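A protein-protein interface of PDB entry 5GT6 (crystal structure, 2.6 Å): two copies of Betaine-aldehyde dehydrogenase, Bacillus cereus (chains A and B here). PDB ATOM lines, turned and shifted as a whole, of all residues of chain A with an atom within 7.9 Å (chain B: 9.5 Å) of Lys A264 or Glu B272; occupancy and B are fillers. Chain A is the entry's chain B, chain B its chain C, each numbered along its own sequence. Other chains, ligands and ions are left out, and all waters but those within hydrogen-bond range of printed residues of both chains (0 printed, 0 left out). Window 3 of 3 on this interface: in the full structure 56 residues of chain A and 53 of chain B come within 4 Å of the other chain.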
ATOM      1  N   PHE A 256     -10.445  11.547 -11.310  1.00  0.00           N
ATOM      2  CA  PHE A 256     -11.660  11.466 -10.530  1.00  0.00           C
ATOM      3  C   PHE A 256     -11.954  12.530  -9.502  1.00  0.00           C
ATOM      4  O   PHE A 256     -11.114  13.002  -8.853  1.00  0.00           O
ATOM      5  CB  PHE A 256     -11.638  10.098  -9.856  1.00  0.00           C
ATOM      6  CG  PHE A 256     -12.729   9.858  -8.880  1.00  0.00           C
ATOM      7  CD1 PHE A 256     -13.936   9.391  -9.287  1.00  0.00           C
ATOM      8  CD2 PHE A 256     -12.526  10.039  -7.535  1.00  0.00           C
ATOM      9  CE1 PHE A 256     -14.924   9.150  -8.380  1.00  0.00           C
ATOM     10  CE2 PHE A 256     -13.512   9.818  -6.637  1.00  0.00           C
ATOM     11  CZ  PHE A 256     -14.712   9.370  -7.053  1.00  0.00           C
ATOM     12  N   SER A 259     -16.110  11.542  -3.484  1.00  0.00           N
ATOM     13  CA  SER A 259     -15.823  11.279  -2.058  1.00  0.00           C
ATOM     14  C   SER A 259     -14.397  10.763  -1.829  1.00  0.00           C
ATOM     15  O   SER A 259     -13.906   9.967  -2.635  1.00  0.00           O
ATOM     16  CB  SER A 259     -16.780  10.222  -1.524  1.00  0.00           C
ATOM     17  OG  SER A 259     -16.589   8.995  -2.226  1.00  0.00           O
ATOM     18  N   THR A 260     -13.773  11.174  -0.720  1.00  0.00           N
ATOM     19  CA  THR A 260     -12.477  10.641  -0.317  1.00  0.00           C
ATOM     20  C   THR A 260     -12.408   9.088  -0.296  1.00  0.00           C
ATOM     21  O   THR A 260     -11.374   8.517  -0.675  1.00  0.00           O
ATOM     22  CB  THR A 260     -11.989  11.274   1.033  1.00  0.00           C
ATOM     23  OG1 THR A 260     -11.669  12.649   0.820  1.00  0.00           O
ATOM     24  CG2 THR A 260     -10.711  10.597   1.584  1.00  0.00           C
ATOM     25  N   VAL A 261     -13.501   8.415   0.086  1.00  0.00           N
ATOM     26  CA  VAL A 261     -13.561   6.927   0.160  1.00  0.00           C
ATOM     27  C   VAL A 261     -13.313   6.256  -1.205  1.00  0.00           C
ATOM     28  O   VAL A 261     -12.557   5.278  -1.288  1.00  0.00           O
ATOM     29  CB  VAL A 261     -14.913   6.428   0.789  1.00  0.00           C
ATOM     30  CG1 VAL A 261     -15.042   4.889   0.767  1.00  0.00           C
ATOM     31  CG2 VAL A 261     -15.070   6.970   2.215  1.00  0.00           C
ATOM     32  N   THR A 262     -13.936   6.779  -2.261  1.00  0.00           N
ATOM     33  CA  THR A 262     -13.801   6.198  -3.622  1.00  0.00           C
ATOM     34  C   THR A 262     -12.464   6.485  -4.288  1.00  0.00           C
ATOM     35  O   THR A 262     -11.993   5.674  -5.095  1.00  0.00           O
ATOM     36  CB  THR A 262     -14.882   6.706  -4.600  1.00  0.00           C
ATOM     37  OG1 THR A 262     -16.132   6.874  -3.923  1.00  0.00           O
ATOM     38  CG2 THR A 262     -15.060   5.740  -5.793  1.00  0.00           C
ATOM     39  N   GLY A 263     -11.907   7.659  -4.002  1.00  0.00           N
ATOM     40  CA  GLY A 263     -10.556   8.028  -4.430  1.00  0.00           C
ATOM     41  C   GLY A 263      -9.486   7.059  -3.939  1.00  0.00           C
ATOM     42  O   GLY A 263      -8.552   6.763  -4.670  1.00  0.00           O
ATOM     43  N   LYS A 264      -9.625   6.557  -2.708  1.00  0.00           N
ATOM     44  CA  LYS A 264      -8.752   5.483  -2.214  1.00  0.00           C
ATOM     45  C   LYS A 264      -8.870   4.231  -3.090  1.00  0.00           C
ATOM     46  O   LYS A 264      -7.844   3.705  -3.542  1.00  0.00           O
ATOM     47  CB  LYS A 264      -9.067   5.109  -0.767  1.00  0.00           C
ATOM     48  CG  LYS A 264      -8.864   6.236   0.198  1.00  0.00           C
ATOM     49  CD  LYS A 264      -9.290   5.878   1.598  1.00  0.00           C
ATOM     50  CE  LYS A 264      -9.095   7.093   2.489  1.00  0.00           C
ATOM     51  NZ  LYS A 264      -8.963   6.728   3.919  1.00  0.00           N
ATOM     52  N   TYR A 265     -10.113   3.778  -3.329  1.00  0.00           N
ATOM     53  CA  TYR A 265     -10.399   2.623  -4.229  1.00  0.00           C
ATOM     54  C   TYR A 265      -9.775   2.791  -5.623  1.00  0.00           C
ATOM     55  O   TYR A 265      -9.050   1.915  -6.113  1.00  0.00           O
ATOM     56  CB  TYR A 265     -11.918   2.371  -4.336  1.00  0.00           C
ATOM     57  CG  TYR A 265     -12.338   1.410  -5.438  1.00  0.00           C
ATOM     58  CD1 TYR A 265     -12.278   0.033  -5.257  1.00  0.00           C
ATOM     59  CD2 TYR A 265     -12.791   1.900  -6.665  1.00  0.00           C
ATOM     60  CE1 TYR A 265     -12.661  -0.828  -6.277  1.00  0.00           C
ATOM     61  CE2 TYR A 265     -13.162   1.053  -7.699  1.00  0.00           C
ATOM     62  CZ  TYR A 265     -13.108  -0.308  -7.506  1.00  0.00           C
ATOM     63  OH  TYR A 265     -13.476  -1.130  -8.553  1.00  0.00           O
ATOM     64  N   ILE A 266     -10.049   3.937  -6.239  1.00  0.00           N
ATOM     65  CA  ILE A 266      -9.483   4.294  -7.540  1.00  0.00           C
ATOM     66  C   ILE A 266      -7.948   4.333  -7.560  1.00  0.00           C
ATOM     67  O   ILE A 266      -7.327   3.925  -8.551  1.00  0.00           O
ATOM     68  CB  ILE A 266     -10.119   5.621  -8.033  1.00  0.00           C
ATOM     69  CG1 ILE A 266     -11.535   5.311  -8.522  1.00  0.00           C
ATOM     70  CG2 ILE A 266      -9.316   6.284  -9.150  1.00  0.00           C
ATOM     71  CD1 ILE A 266     -12.442   6.486  -8.505  1.00  0.00           C
ATOM     72  N   MET A 267      -7.342   4.798  -6.473  1.00  0.00           N
ATOM     73  CA  MET A 267      -5.885   4.810  -6.361  1.00  0.00           C
ATOM     74  C   MET A 267      -5.304   3.400  -6.117  1.00  0.00           C
ATOM     75  O   MET A 267      -4.241   3.065  -6.648  1.00  0.00           O
ATOM     76  CB  MET A 267      -5.430   5.789  -5.280  1.00  0.00           C
ATOM     77  CG  MET A 267      -3.964   6.148  -5.412  1.00  0.00           C
ATOM     78  SD  MET A 267      -3.361   7.431  -4.294  1.00  0.00           S
ATOM     79  CE  MET A 267      -1.674   7.483  -4.926  1.00  0.00           C
ATOM     80  N   ARG A 268      -6.014   2.591  -5.332  1.00  0.00           N
ATOM     81  CA  ARG A 268      -5.682   1.169  -5.112  1.00  0.00           C
ATOM     82  C   ARG A 268      -5.768   0.393  -6.433  1.00  0.00           C
ATOM     83  O   ARG A 268      -4.815  -0.300  -6.810  1.00  0.00           O
ATOM     84  CB  ARG A 268      -6.612   0.557  -4.050  1.00  0.00           C
ATOM     85  CG  ARG A 268      -6.135  -0.753  -3.430  1.00  0.00           C
ATOM     86  CD  ARG A 268      -7.108  -1.315  -2.397  1.00  0.00           C
ATOM     87  NE  ARG A 268      -7.580  -0.253  -1.496  1.00  0.00           N
ATOM     88  CZ  ARG A 268      -8.833   0.244  -1.419  1.00  0.00           C
ATOM     89  NH1 ARG A 268      -9.847  -0.210  -2.173  1.00  0.00           N
ATOM     90  NH2 ARG A 268      -9.085   1.229  -0.554  1.00  0.00           N
ATOM     91  N   GLN A 269      -6.880   0.544  -7.155  1.00  0.00           N
ATOM     92  CA  GLN A 269      -7.072  -0.168  -8.436  1.00  0.00           C
ATOM     93  C   GLN A 269      -6.116   0.319  -9.519  1.00  0.00           C
ATOM     94  O   GLN A 269      -5.676  -0.458 -10.364  1.00  0.00           O
ATOM     95  CB  GLN A 269      -8.529  -0.048  -8.917  1.00  0.00           C
ATOM     96  CG  GLN A 269      -9.547  -0.728  -7.998  1.00  0.00           C
ATOM     97  CD  GLN A 269      -9.307  -2.208  -7.917  1.00  0.00           C
ATOM     98  OE1 GLN A 269      -8.819  -2.708  -6.907  1.00  0.00           O
ATOM     99  NE2 GLN A 269      -9.581  -2.909  -8.999  1.00  0.00           N
ATOM    100  N   SER A 270      -5.763   1.597  -9.481  1.00  0.00           N
ATOM    101  CA  SER A 270      -4.804   2.118 -10.447  1.00  0.00           C
ATOM    102  C   SER A 270      -3.369   1.610 -10.256  1.00  0.00           C
ATOM    103  O   SER A 270      -2.558   1.751 -11.159  1.00  0.00           O
ATOM    104  CB  SER A 270      -4.869   3.637 -10.458  1.00  0.00           C
ATOM    105  OG  SER A 270      -6.166   4.054 -10.887  1.00  0.00           O
ATOM    106  N   ALA A 271      -3.079   0.997  -9.101  1.00  0.00           N
ATOM    107  CA  ALA A 271      -1.748   0.474  -8.750  1.00  0.00           C
ATOM    108  C   ALA A 271      -1.346  -0.759  -9.539  1.00  0.00           C
ATOM    109  O   ALA A 271      -0.159  -0.978  -9.742  1.00  0.00           O
ATOM    110  CB  ALA A 271      -1.670   0.168  -7.259  1.00  0.00           C
ATOM    111  N   LEU A 279      -6.855  13.193  -8.360  1.00  0.00           N
ATOM    112  CA  LEU A 279      -7.992  13.079  -7.502  1.00  0.00           C
ATOM    113  C   LEU A 279      -8.390  14.364  -6.885  1.00  0.00           C
ATOM    114  O   LEU A 279      -7.595  15.024  -6.356  1.00  0.00           O
ATOM    115  CB  LEU A 279      -7.679  12.130  -6.368  1.00  0.00           C
ATOM    116  CG  LEU A 279      -7.153  10.740  -6.611  1.00  0.00           C
ATOM    117  CD1 LEU A 279      -6.671  10.191  -5.296  1.00  0.00           C
ATOM    118  CD2 LEU A 279      -8.277   9.907  -7.166  1.00  0.00           C
ATOM    119  N   LEU A 281     -11.028  15.507  -4.110  1.00  0.00           N
ATOM    120  CA  LEU A 281     -11.937  14.961  -3.112  1.00  0.00           C
ATOM    121  C   LEU A 281     -12.598  15.912  -2.125  1.00  0.00           C
ATOM    122  O   LEU A 281     -12.706  17.071  -2.399  1.00  0.00           O
ATOM    123  CB  LEU A 281     -11.269  13.804  -2.397  1.00  0.00           C
ATOM    124  CG  LEU A 281     -10.317  12.889  -3.135  1.00  0.00           C
ATOM    125  CD1 LEU A 281      -9.650  12.001  -2.153  1.00  0.00           C
ATOM    126  CD2 LEU A 281     -10.971  12.033  -4.175  1.00  0.00           C
ATOM    127  N   SER A 436      -7.869  15.972   8.375  1.00  0.00           N
ATOM    128  CA  SER A 436      -7.394  15.148   7.282  1.00  0.00           C
ATOM    129  C   SER A 436      -7.629  15.811   5.956  1.00  0.00           C
ATOM    130  O   SER A 436      -7.018  15.418   4.960  1.00  0.00           O
ATOM    131  CB  SER A 436      -8.080  13.778   7.286  1.00  0.00           C
ATOM    132  OG  SER A 436      -7.286  12.893   8.054  1.00  0.00           O
ATOM    133  N   GLN A 482      -5.626  14.525   2.412  1.00  0.00           N
ATOM    134  CA  GLN A 482      -6.550  13.605   1.827  1.00  0.00           C
ATOM    135  C   GLN A 482      -7.641  14.283   1.012  1.00  0.00           C
ATOM    136  O   GLN A 482      -8.583  13.696   0.658  1.00  0.00           O
ATOM    137  CB  GLN A 482      -7.085  12.630   2.868  1.00  0.00           C
ATOM    138  CG  GLN A 482      -6.024  12.110   3.794  1.00  0.00           C
ATOM    139  CD  GLN A 482      -6.377  10.844   4.518  1.00  0.00           C
ATOM    140  OE1 GLN A 482      -7.276  10.153   4.170  1.00  0.00           O
ATOM    141  NE2 GLN A 482      -5.643  10.548   5.528  1.00  0.00           N
ATOM    142  N   VAL B 246       6.112   3.513   4.222  1.00  0.00           N
ATOM    143  CA  VAL B 246       5.009   3.660   3.300  1.00  0.00           C
ATOM    144  C   VAL B 246       3.623   3.719   4.014  1.00  0.00           C
ATOM    145  O   VAL B 246       2.719   4.432   3.549  1.00  0.00           O
ATOM    146  CB  VAL B 246       5.134   2.652   2.116  1.00  0.00           C
ATOM    147  CG1 VAL B 246       4.506   1.299   2.427  1.00  0.00           C
ATOM    148  CG2 VAL B 246       4.540   3.274   0.864  1.00  0.00           C
ATOM    149  N   ASN B 247       3.496   3.059   5.166  1.00  0.00           N
ATOM    150  CA  ASN B 247       2.229   3.042   5.941  1.00  0.00           C
ATOM    151  C   ASN B 247       2.097   4.119   7.026  1.00  0.00           C
ATOM    152  O   ASN B 247       1.100   4.117   7.739  1.00  0.00           O
ATOM    153  CB  ASN B 247       2.027   1.661   6.605  1.00  0.00           C
ATOM    154  CG  ASN B 247       1.917   0.546   5.587  1.00  0.00           C
ATOM    155  OD1 ASN B 247       1.126   0.604   4.648  1.00  0.00           O
ATOM    156  ND2 ASN B 247       2.750  -0.444   5.741  1.00  0.00           N
ATOM    157  N   HIS B 248       3.082   5.020   7.145  1.00  0.00           N
ATOM    158  CA  HIS B 248       3.168   5.913   8.281  1.00  0.00           C
ATOM    159  C   HIS B 248       2.204   7.087   8.104  1.00  0.00           C
ATOM    160  O   HIS B 248       2.202   7.742   7.045  1.00  0.00           O
ATOM    161  CB  HIS B 248       4.596   6.421   8.455  1.00  0.00           C
ATOM    162  CG  HIS B 248       4.864   6.974   9.806  1.00  0.00           C
ATOM    163  ND1 HIS B 248       4.404   8.200  10.193  1.00  0.00           N
ATOM    164  CD2 HIS B 248       5.522   6.471  10.864  1.00  0.00           C
ATOM    165  CE1 HIS B 248       4.774   8.444  11.436  1.00  0.00           C
ATOM    166  NE2 HIS B 248       5.455   7.404  11.867  1.00  0.00           N
ATOM    167  N   HIS B 249       1.430   7.362   9.157  1.00  0.00           N
ATOM    168  CA  HIS B 249       0.352   8.360   9.128  1.00  0.00           C
ATOM    169  C   HIS B 249       0.852   9.810   8.950  1.00  0.00           C
ATOM    170  O   HIS B 249       0.179  10.619   8.326  1.00  0.00           O
ATOM    171  CB  HIS B 249      -0.521   8.241  10.402  1.00  0.00           C
ATOM    172  CG  HIS B 249       0.082   8.867  11.636  1.00  0.00           C
ATOM    173  ND1 HIS B 249       0.864   8.160  12.530  1.00  0.00           N
ATOM    174  CD2 HIS B 249       0.010  10.137  12.124  1.00  0.00           C
ATOM    175  CE1 HIS B 249       1.256   8.968  13.506  1.00  0.00           C
ATOM    176  NE2 HIS B 249       0.747  10.172  13.284  1.00  0.00           N
ATOM    177  N   TYR B 265       2.662  -2.446  -4.713  1.00  0.00           N
ATOM    178  CA  TYR B 265       2.425  -2.513  -3.260  1.00  0.00           C
ATOM    179  C   TYR B 265       2.517  -1.097  -2.676  1.00  0.00           C
ATOM    180  O   TYR B 265       1.624  -0.641  -1.942  1.00  0.00           O
ATOM    181  CB  TYR B 265       3.426  -3.493  -2.566  1.00  0.00           C
ATOM    182  CG  TYR B 265       3.569  -3.293  -1.056  1.00  0.00           C
ATOM    183  CD1 TYR B 265       2.590  -3.770  -0.180  1.00  0.00           C
ATOM    184  CD2 TYR B 265       4.662  -2.590  -0.513  1.00  0.00           C
ATOM    185  CE1 TYR B 265       2.684  -3.559   1.184  1.00  0.00           C
ATOM    186  CE2 TYR B 265       4.771  -2.372   0.861  1.00  0.00           C
ATOM    187  CZ  TYR B 265       3.779  -2.864   1.708  1.00  0.00           C
ATOM    188  OH  TYR B 265       3.846  -2.680   3.069  1.00  0.00           O
ATOM    189  N   ILE B 266       3.582  -0.384  -3.034  1.00  0.00           N
ATOM    190  CA  ILE B 266       3.759   0.976  -2.551  1.00  0.00           C
ATOM    191  C   ILE B 266       2.630   1.937  -2.934  1.00  0.00           C
ATOM    192  O   ILE B 266       2.247   2.769  -2.128  1.00  0.00           O
ATOM    193  CB  ILE B 266       5.139   1.523  -2.922  1.00  0.00           C
ATOM    194  CG1 ILE B 266       6.128   0.944  -1.910  1.00  0.00           C
ATOM    195  CG2 ILE B 266       5.150   3.047  -2.888  1.00  0.00           C
ATOM    196  CD1 ILE B 266       7.548   1.376  -2.121  1.00  0.00           C
ATOM    197  N   MET B 267       2.088   1.795  -4.130  1.00  0.00           N
ATOM    198  CA  MET B 267       0.961   2.618  -4.571  1.00  0.00           C
ATOM    199  C   MET B 267      -0.368   2.186  -3.936  1.00  0.00           C
ATOM    200  O   MET B 267      -1.158   3.046  -3.546  1.00  0.00           O
ATOM    201  CB  MET B 267       0.876   2.611  -6.099  1.00  0.00           C
ATOM    202  CG  MET B 267       0.145   3.800  -6.674  1.00  0.00           C
ATOM    203  SD  MET B 267       0.147   3.785  -8.476  1.00  0.00           S
ATOM    204  CE  MET B 267      -1.259   4.862  -8.736  1.00  0.00           C
ATOM    205  N   ARG B 268      -0.610   0.876  -3.844  1.00  0.00           N
ATOM    206  CA  ARG B 268      -1.754   0.320  -3.059  1.00  0.00           C
ATOM    207  C   ARG B 268      -1.861   0.861  -1.630  1.00  0.00           C
ATOM    208  O   ARG B 268      -2.961   1.185  -1.173  1.00  0.00           O
ATOM    209  CB  ARG B 268      -1.676  -1.209  -2.940  1.00  0.00           C
ATOM    210  CG  ARG B 268      -2.464  -2.016  -3.960  1.00  0.00           C
ATOM    211  CD  ARG B 268      -2.288  -3.515  -3.699  1.00  0.00           C
ATOM    212  NE  ARG B 268      -1.097  -4.021  -4.394  1.00  0.00           N
ATOM    213  CZ  ARG B 268      -0.287  -5.003  -3.982  1.00  0.00           C
ATOM    214  NH1 ARG B 268      -0.477  -5.652  -2.831  1.00  0.00           N
ATOM    215  NH2 ARG B 268       0.752  -5.326  -4.743  1.00  0.00           N
ATOM    216  N   GLN B 269      -0.723   0.930  -0.933  1.00  0.00           N
ATOM    217  CA  GLN B 269      -0.682   1.372   0.483  1.00  0.00           C
ATOM    218  C   GLN B 269      -0.725   2.894   0.664  1.00  0.00           C
ATOM    219  O   GLN B 269      -1.304   3.403   1.638  1.00  0.00           O
ATOM    220  CB  GLN B 269       0.554   0.807   1.202  1.00  0.00           C
ATOM    221  CG  GLN B 269       0.716  -0.720   1.159  1.00  0.00           C
ATOM    222  CD  GLN B 269      -0.423  -1.477   1.812  1.00  0.00           C
ATOM    223  OE1 GLN B 269      -1.206  -2.188   1.137  1.00  0.00           O
ATOM    224  NE2 GLN B 269      -0.545  -1.311   3.121  1.00  0.00           N
ATOM    225  N   SER B 270      -0.078   3.601  -0.261  1.00  0.00           N
ATOM    226  CA  SER B 270      -0.173   5.053  -0.361  1.00  0.00           C
ATOM    227  C   SER B 270      -1.608   5.531  -0.535  1.00  0.00           C
ATOM    228  O   SER B 270      -1.962   6.594  -0.025  1.00  0.00           O
ATOM    229  CB  SER B 270       0.657   5.561  -1.521  1.00  0.00           C
ATOM    230  OG  SER B 270       2.010   5.417  -1.203  1.00  0.00           O
ATOM    231  N   ALA B 271      -2.414   4.733  -1.243  1.00  0.00           N
ATOM    232  CA  ALA B 271      -3.863   4.999  -1.463  1.00  0.00           C
ATOM    233  C   ALA B 271      -4.675   5.216  -0.197  1.00  0.00           C
ATOM    234  O   ALA B 271      -5.542   6.077  -0.178  1.00  0.00           O
ATOM    235  CB  ALA B 271      -4.501   3.882  -2.278  1.00  0.00           C
ATOM    236  N   GLU B 272      -4.390   4.470   0.861  1.00  0.00           N
ATOM    237  CA  GLU B 272      -5.147   4.645   2.106  1.00  0.00           C
ATOM    238  C   GLU B 272      -5.164   6.083   2.630  1.00  0.00           C
ATOM    239  O   GLU B 272      -6.083   6.449   3.323  1.00  0.00           O
ATOM    240  CB  GLU B 272      -4.692   3.658   3.192  1.00  0.00           C
ATOM    241  CG  GLU B 272      -5.432   2.312   3.129  1.00  0.00           C
ATOM    242  CD  GLU B 272      -6.775   2.334   3.891  1.00  0.00           C
ATOM    243  OE1 GLU B 272      -7.626   3.221   3.630  1.00  0.00           O
ATOM    244  OE2 GLU B 272      -6.978   1.465   4.776  1.00  0.00           O
ATOM    245  N   MET B 273      -4.170   6.889   2.248  1.00  0.00           N
ATOM    246  CA  MET B 273      -3.990   8.269   2.732  1.00  0.00           C
ATOM    247  C   MET B 273      -3.896   9.385   1.686  1.00  0.00           C
ATOM    248  O   MET B 273      -3.499  10.507   1.991  1.00  0.00           O
ATOM    249  CB  MET B 273      -2.759   8.256   3.608  1.00  0.00           C
ATOM    250  CG  MET B 273      -3.045   7.411   4.830  1.00  0.00           C
ATOM    251  SD  MET B 273      -1.684   7.420   5.946  1.00  0.00           S
ATOM    252  CE  MET B 273      -0.601   6.238   5.080  1.00  0.00           C
ATOM    253  N   ILE B 274      -4.326   9.076   0.469  1.00  0.00           N
ATOM    254  CA  ILE B 274      -4.240   9.978  -0.679  1.00  0.00           C
ATOM    255  C   ILE B 274      -2.869  10.675  -0.655  1.00  0.00           C
ATOM    256  O   ILE B 274      -2.740  11.901  -0.720  1.00  0.00           O
ATOM    257  CB  ILE B 274      -5.506  10.885  -0.775  1.00  0.00           C
ATOM    258  CG1 ILE B 274      -6.767  10.009  -0.893  1.00  0.00           C
ATOM    259  CG2 ILE B 274      -5.496  11.761  -2.013  1.00  0.00           C
ATOM    260  CD1 ILE B 274      -7.544   9.867   0.381  1.00  0.00           C
ATOM    261  N   LYS B 275      -1.851   9.819  -0.561  1.00  0.00           N
ATOM    262  CA  LYS B 275      -0.438  10.183  -0.564  1.00  0.00           C
ATOM    263  C   LYS B 275       0.104  10.153  -2.029  1.00  0.00           C
ATOM    264  O   LYS B 275      -0.013   9.130  -2.744  1.00  0.00           O
ATOM    265  CB  LYS B 275       0.322   9.191   0.327  1.00  0.00           C
ATOM    266  CG  LYS B 275       1.620   9.701   0.913  1.00  0.00           C
ATOM    267  CD  LYS B 275       2.280   8.720   1.886  1.00  0.00           C
ATOM    268  CE  LYS B 275       1.442   8.457   3.132  1.00  0.00           C
ATOM    269  NZ  LYS B 275       2.282   7.962   4.258  1.00  0.00           N
ATOM    270  N   HIS B 276       0.757  11.223  -2.459  1.00  0.00           N
ATOM    271  CA  HIS B 276       1.402  11.338  -3.763  1.00  0.00           C
ATOM    272  C   HIS B 276       2.502  10.310  -3.880  1.00  0.00           C
ATOM    273  O   HIS B 276       3.139   9.995  -2.926  1.00  0.00           O
ATOM    274  CB  HIS B 276       2.031  12.705  -3.826  1.00  0.00           C
ATOM    275  CG  HIS B 276       2.636  13.079  -5.138  1.00  0.00           C
ATOM    276  ND1 HIS B 276       1.957  13.813  -6.066  1.00  0.00           N
ATOM    277  CD2 HIS B 276       3.879  12.916  -5.634  1.00  0.00           C
ATOM    278  CE1 HIS B 276       2.735  14.036  -7.097  1.00  0.00           C
ATOM    279  NE2 HIS B 276       3.904  13.498  -6.856  1.00  0.00           N
ATOM    280  N   VAL B 277       2.703   9.783  -5.064  1.00  0.00           N
ATOM    281  CA  VAL B 277       3.709   8.794  -5.305  1.00  0.00           C
ATOM    282  C   VAL B 277       4.444   9.080  -6.551  1.00  0.00           C
ATOM    283  O   VAL B 277       3.886   9.420  -7.536  1.00  0.00           O
ATOM    284  CB  VAL B 277       3.106   7.380  -5.485  1.00  0.00           C
ATOM    285  CG1 VAL B 277       4.140   6.295  -5.426  1.00  0.00           C
ATOM    286  CG2 VAL B 277       2.118   7.106  -4.435  1.00  0.00           C
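Printed residues of chain A that touch a printed residue of chain B: Thr A260, Lys A264, Met A267, Arg A268, Ala A271, Leu A279, Leu A281 and Gln A482.
Hydrophobic or aromatic side chains of chain A within 4 Å of the printed part of chain B: Met A267, Ala A271, Leu A279 and Leu A281.
Of the 17 printed residues of chain B, 8 touch a printed residue of chain A.
Hydrophobic or aromatic side chains of chain B that line the printed part of chain A: Met B267, Ala B271, Ile B274 and Val B277.
Along chain B the printed residues that touch a printed residue of chain A span positions 267 to 277.
Among the printed residues, 16 pairs touch across the chains.
Among the printed residues, merely in contact across the chains: Met A267 with Lys B275 (3.2 Å), Lys A264 with Ala B271 (3.3 Å), Thr A260 with Ile B274 (3.5 Å), Gln A482 with Met B273 (3.5 Å), Arg A268 with Ala B271 (3.6 Å), Ala A271 with Arg B268 (3.6 Å), Met A267 with Ala B271 (3.7 Å), Ala A271 with Met B267 (3.7 Å), Leu A281 with Ile B274 (3.7 Å), Gln A482 with Ile B274 (3.7 Å), Lys A264 with Ile B274 (3.8 Å), Leu A279 with Ile B274 (3.8 Å), Met A267 with Val B277 (3.8 Å), Arg A268 with Arg B268 (3.9 Å) and Gln A482 with Glu B272 (3.98 Å).
OG1 of Thr A260 is in hydrogen-bond range of O of Gln A482, 3.3 Å away.
N of Gln A482 is in hydrogen-bond range of O of Ser A436, 3.0 Å away.
The side-chain amino group (NZ) of Lys B275 lies within hydrogen-bond range of the backbone carbonyl oxygen (O) of His B248, 2.8 Å away.
The backbone carbonyl oxygen of Ser B270 lies within hydrogen-bond range of the backbone NH of Lys B275 (3.3 Å).
Met A267 touches Ala B271, and with the chains exchanged Ala A271 touches Met B267.
Arg A268 touches its own counterpart, Arg B268.
Arg A268 touches Ala B271, and with the chains exchanged Ala A271 touches Arg B268.
NZ of Lys A264 is in salt-bridge range of OE1 of Glu B272, 3.8 Å away.
Of the printed residues of chain B, Thr A260 touches Ile B274.
No residue of chain B comes within 4 Å of Gly A263.
Of the printed residues of chain B, Lys A264 touches Ala B271, Glu B272 and Ile B274.
Gln A269 touches none of the printed residues of chain B.
Printed residues of chain B within 4 Å of Leu A281: Ile B274.
The nearest residue of chain B that does not touch Lys A264 is Met B273 (4.9 Å).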
